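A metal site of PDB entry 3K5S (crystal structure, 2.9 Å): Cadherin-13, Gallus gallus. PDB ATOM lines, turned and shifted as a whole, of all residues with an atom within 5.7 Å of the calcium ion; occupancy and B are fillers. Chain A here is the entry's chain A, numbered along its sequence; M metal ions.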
ATOM      1  N   ASN A 101       3.010  -5.436 -26.840  1.00  0.00           N
ATOM      2  CA  ASN A 101       3.595  -6.778 -26.846  1.00  0.00           C
ATOM      3  C   ASN A 101       2.852  -7.776 -27.753  1.00  0.00           C
ATOM      4  O   ASN A 101       2.028  -8.550 -27.293  1.00  0.00           O
ATOM      5  CB  ASN A 101       3.670  -7.317 -25.412  1.00  0.00           C
ATOM      6  CG  ASN A 101       4.625  -8.492 -25.283  1.00  0.00           C
ATOM      7  OD1 ASN A 101       5.677  -8.513 -25.921  1.00  0.00           O
ATOM      8  ND2 ASN A 101       4.262  -9.477 -24.461  1.00  0.00           N
ATOM      9  N   ASP A 102       3.152  -7.761 -29.042  1.00  0.00           N
ATOM     10  CA  ASP A 102       2.410  -8.584 -29.980  1.00  0.00           C
ATOM     11  C   ASP A 102       3.272  -9.513 -30.796  1.00  0.00           C
ATOM     12  O   ASP A 102       2.829 -10.054 -31.806  1.00  0.00           O
ATOM     13  CB  ASP A 102       1.502  -7.736 -30.894  1.00  0.00           C
ATOM     14  CG  ASP A 102       2.271  -6.708 -31.710  1.00  0.00           C
ATOM     15  OD1 ASP A 102       3.476  -6.906 -31.966  1.00  0.00           O
ATOM     16  OD2 ASP A 102       1.646  -5.708 -32.104  1.00  0.00           O
ATOM     17  N   ASN A 103       4.495  -9.706 -30.362  1.00  0.00           N
ATOM     18  CA  ASN A 103       5.334 -10.692 -31.007  1.00  0.00           C
ATOM     19  C   ASN A 103       5.840 -11.685 -29.980  1.00  0.00           C
ATOM     20  O   ASN A 103       6.334 -11.293 -28.942  1.00  0.00           O
ATOM     21  CB  ASN A 103       6.500 -10.038 -31.736  1.00  0.00           C
ATOM     22  CG  ASN A 103       6.108  -9.509 -33.093  1.00  0.00           C
ATOM     23  OD1 ASN A 103       5.901 -10.282 -34.031  1.00  0.00           O
ATOM     24  ND2 ASN A 103       6.022  -8.193 -33.215  1.00  0.00           N
ATOM     25  N   ARG A 104       5.704 -12.964 -30.257  1.00  0.00           N
ATOM     26  CA  ARG A 104       6.104 -13.954 -29.263  1.00  0.00           C
ATOM     27  C   ARG A 104       7.588 -14.288 -29.446  1.00  0.00           C
ATOM     28  O   ARG A 104       8.066 -14.383 -30.570  1.00  0.00           O
ATOM     29  CB  ARG A 104       5.202 -15.190 -29.391  1.00  0.00           C
ATOM     30  CG  ARG A 104       5.803 -16.473 -28.863  1.00  0.00           C
ATOM     31  CD  ARG A 104       5.173 -17.686 -29.538  1.00  0.00           C
ATOM     32  NE  ARG A 104       3.757 -17.444 -29.820  1.00  0.00           N
ATOM     33  CZ  ARG A 104       2.789 -17.577 -28.921  1.00  0.00           C
ATOM     34  NH1 ARG A 104       3.080 -17.934 -27.669  1.00  0.00           N
ATOM     35  NH2 ARG A 104       1.518 -17.336 -29.264  1.00  0.00           N
ATOM     36  N   PRO A 105       8.331 -14.434 -28.330  1.00  0.00           N
ATOM     37  CA  PRO A 105       9.746 -14.858 -28.397  1.00  0.00           C
ATOM     38  C   PRO A 105       9.912 -16.160 -29.183  1.00  0.00           C
ATOM     39  O   PRO A 105       9.132 -17.101 -28.977  1.00  0.00           O
ATOM     40  CB  PRO A 105      10.095 -15.106 -26.918  1.00  0.00           C
ATOM     41  CG  PRO A 105       9.134 -14.332 -26.126  1.00  0.00           C
ATOM     42  CD  PRO A 105       7.869 -14.252 -26.945  1.00  0.00           C
ATOM     43  N   ASP A 133      13.133 -11.735 -30.402  1.00  0.00           N
ATOM     44  CA  ASP A 133      11.791 -11.202 -30.156  1.00  0.00           C
ATOM     45  C   ASP A 133      11.540  -9.943 -30.977  1.00  0.00           C
ATOM     46  O   ASP A 133      12.216  -8.940 -30.805  1.00  0.00           O
ATOM     47  CB  ASP A 133      11.624 -10.882 -28.670  1.00  0.00           C
ATOM     48  CG  ASP A 133      10.185 -10.643 -28.296  1.00  0.00           C
ATOM     49  OD1 ASP A 133       9.539  -9.767 -28.904  1.00  0.00           O
ATOM     50  OD2 ASP A 133       9.694 -11.347 -27.379  1.00  0.00           O
ATOM     51  N   ALA A 134      10.544  -9.999 -31.860  1.00  0.00           N
ATOM     52  CA  ALA A 134      10.317  -8.911 -32.800  1.00  0.00           C
ATOM     53  C   ALA A 134       9.990  -7.554 -32.167  1.00  0.00           C
ATOM     54  O   ALA A 134      10.026  -6.521 -32.842  1.00  0.00           O
ATOM     55  CB  ALA A 134       9.252  -9.286 -33.820  1.00  0.00           C
ATOM     56  N   ASP A 135       9.679  -7.547 -30.878  1.00  0.00           N
ATOM     57  CA  ASP A 135       9.242  -6.321 -30.201  1.00  0.00           C
ATOM     58  C   ASP A 135      10.394  -5.393 -29.778  1.00  0.00           C
ATOM     59  O   ASP A 135      11.529  -5.573 -30.215  1.00  0.00           O
ATOM     60  CB  ASP A 135       8.290  -6.647 -29.056  1.00  0.00           C
ATOM     61  CG  ASP A 135       6.968  -7.227 -29.553  1.00  0.00           C
ATOM     62  OD1 ASP A 135       6.797  -7.357 -30.780  1.00  0.00           O
ATOM     63  OD2 ASP A 135       6.094  -7.558 -28.733  1.00  0.00           O
ATOM     64  N   ASN A 141       8.504  -5.686 -23.650  1.00  0.00           N
ATOM     65  CA  ASN A 141       7.819  -6.522 -24.605  1.00  0.00           C
ATOM     66  C   ASN A 141       8.796  -7.512 -25.222  1.00  0.00           C
ATOM     67  O   ASN A 141       8.460  -8.654 -25.452  1.00  0.00           O
ATOM     68  CB  ASN A 141       7.050  -5.675 -25.597  1.00  0.00           C
ATOM     69  CG  ASN A 141       6.052  -4.748 -24.918  1.00  0.00           C
ATOM     70  OD1 ASN A 141       5.809  -4.862 -23.719  1.00  0.00           O
ATOM     71  ND2 ASN A 141       5.475  -3.843 -25.680  1.00  0.00           N
ATOM     72  N   ALA A 142      10.021  -7.063 -25.475  1.00  0.00           N
ATOM     73  CA  ALA A 142      11.162  -7.962 -25.526  1.00  0.00           C
ATOM     74  C   ALA A 142      11.791  -7.767 -24.153  1.00  0.00           C
ATOM     75  O   ALA A 142      11.178  -7.148 -23.310  1.00  0.00           O
ATOM     76  CB  ALA A 142      12.112  -7.581 -26.627  1.00  0.00           C
ATOM     77  N   LEU A 144      13.849 -10.822 -22.439  1.00  0.00           N
ATOM     78  CA  LEU A 144      13.510 -12.206 -22.228  1.00  0.00           C
ATOM     79  C   LEU A 144      14.208 -12.785 -20.988  1.00  0.00           C
ATOM     80  O   LEU A 144      15.300 -12.348 -20.601  1.00  0.00           O
ATOM     81  CB  LEU A 144      13.860 -13.001 -23.486  1.00  0.00           C
ATOM     82  CG  LEU A 144      13.593 -12.292 -24.828  1.00  0.00           C
ATOM     83  CD1 LEU A 144      13.755 -13.260 -25.994  1.00  0.00           C
ATOM     84  CD2 LEU A 144      12.227 -11.610 -24.907  1.00  0.00           C
ATOM     85  N   ASP A 197       8.760 -13.435 -22.119  1.00  0.00           N
ATOM     86  CA  ASP A 197       8.682 -11.975 -22.228  1.00  0.00           C
ATOM     87  C   ASP A 197       8.586 -11.268 -20.882  1.00  0.00           C
ATOM     88  O   ASP A 197       8.514 -11.907 -19.830  1.00  0.00           O
ATOM     89  CB  ASP A 197       7.409 -11.602 -22.969  1.00  0.00           C
ATOM     90  CG  ASP A 197       7.648 -11.276 -24.383  1.00  0.00           C
ATOM     91  OD1 ASP A 197       8.835 -11.240 -24.772  1.00  0.00           O
ATOM     92  OD2 ASP A 197       6.655 -11.048 -25.086  1.00  0.00           O
ATOM     93  N   LEU A 205       4.850 -13.918 -22.768  1.00  0.00           N
ATOM     94  CA  LEU A 205       4.583 -14.841 -23.861  1.00  0.00           C
ATOM     95  C   LEU A 205       5.818 -15.718 -23.982  1.00  0.00           C
ATOM     96  O   LEU A 205       6.900 -15.306 -23.566  1.00  0.00           O
ATOM     97  CB  LEU A 205       4.336 -14.079 -25.166  1.00  0.00           C
ATOM     98  CG  LEU A 205       3.040 -13.271 -25.293  1.00  0.00           C
ATOM     99  CD1 LEU A 205       3.221 -12.148 -26.300  1.00  0.00           C
ATOM    100  CD2 LEU A 205       1.847 -14.169 -25.650  1.00  0.00           C
HETATM  101 CA    CA M   1       7.394  -9.939 -27.270  1.00  0.00          CA
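The side-chain carboxylate (OD2) of Asp 135 is in hydrogen-bond range of the backbone NH (N) of Asn 103 (3.1 Å).
The side-chain amide nitrogen (ND2) of Asn 103 sits close to the side-chain carboxylate (OD1) of Asp 102 (3.1 Å).
The backbone NH of Asp 197 sits at hydrogen-bond distance from the backbone carbonyl oxygen of Leu 205 (3.0 Å).
The side-chain carboxylate of Asp 135 sits close to the side-chain amide oxygen of Asn 101 (3.0 Å).
OD1 of Asp 133 sits close to N of Asp 135, 3.0 Å away.
Six residues have an atom within 4 Å of the calcium ion: Asn 101, Asn 103, Asp 133, Asp 135, Asn 141 and Asp 197.
O of Asn 103 is bound to the calcium ion (2.4 Å).
The calcium ion is bound by the backbone carbonyl oxygen (O) of Asn 141, 2.5 Å away.
OD2 of Asp 197 binds the calcium ion, at 2.6 Å.
OD1 of Asn 101 binds the calcium ion (2.6 Å).
The calcium ion is bound by the side-chain carboxylate (OD2) of Asp 133 (2.7 Å).
OD1 of Asp 133 binds the calcium ion (2.7 Å).
The calcium ion has six donor atoms within binding distance.
Slightly farther from the calcium ion lies OD2 of Asp 135 (3.1 Å).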
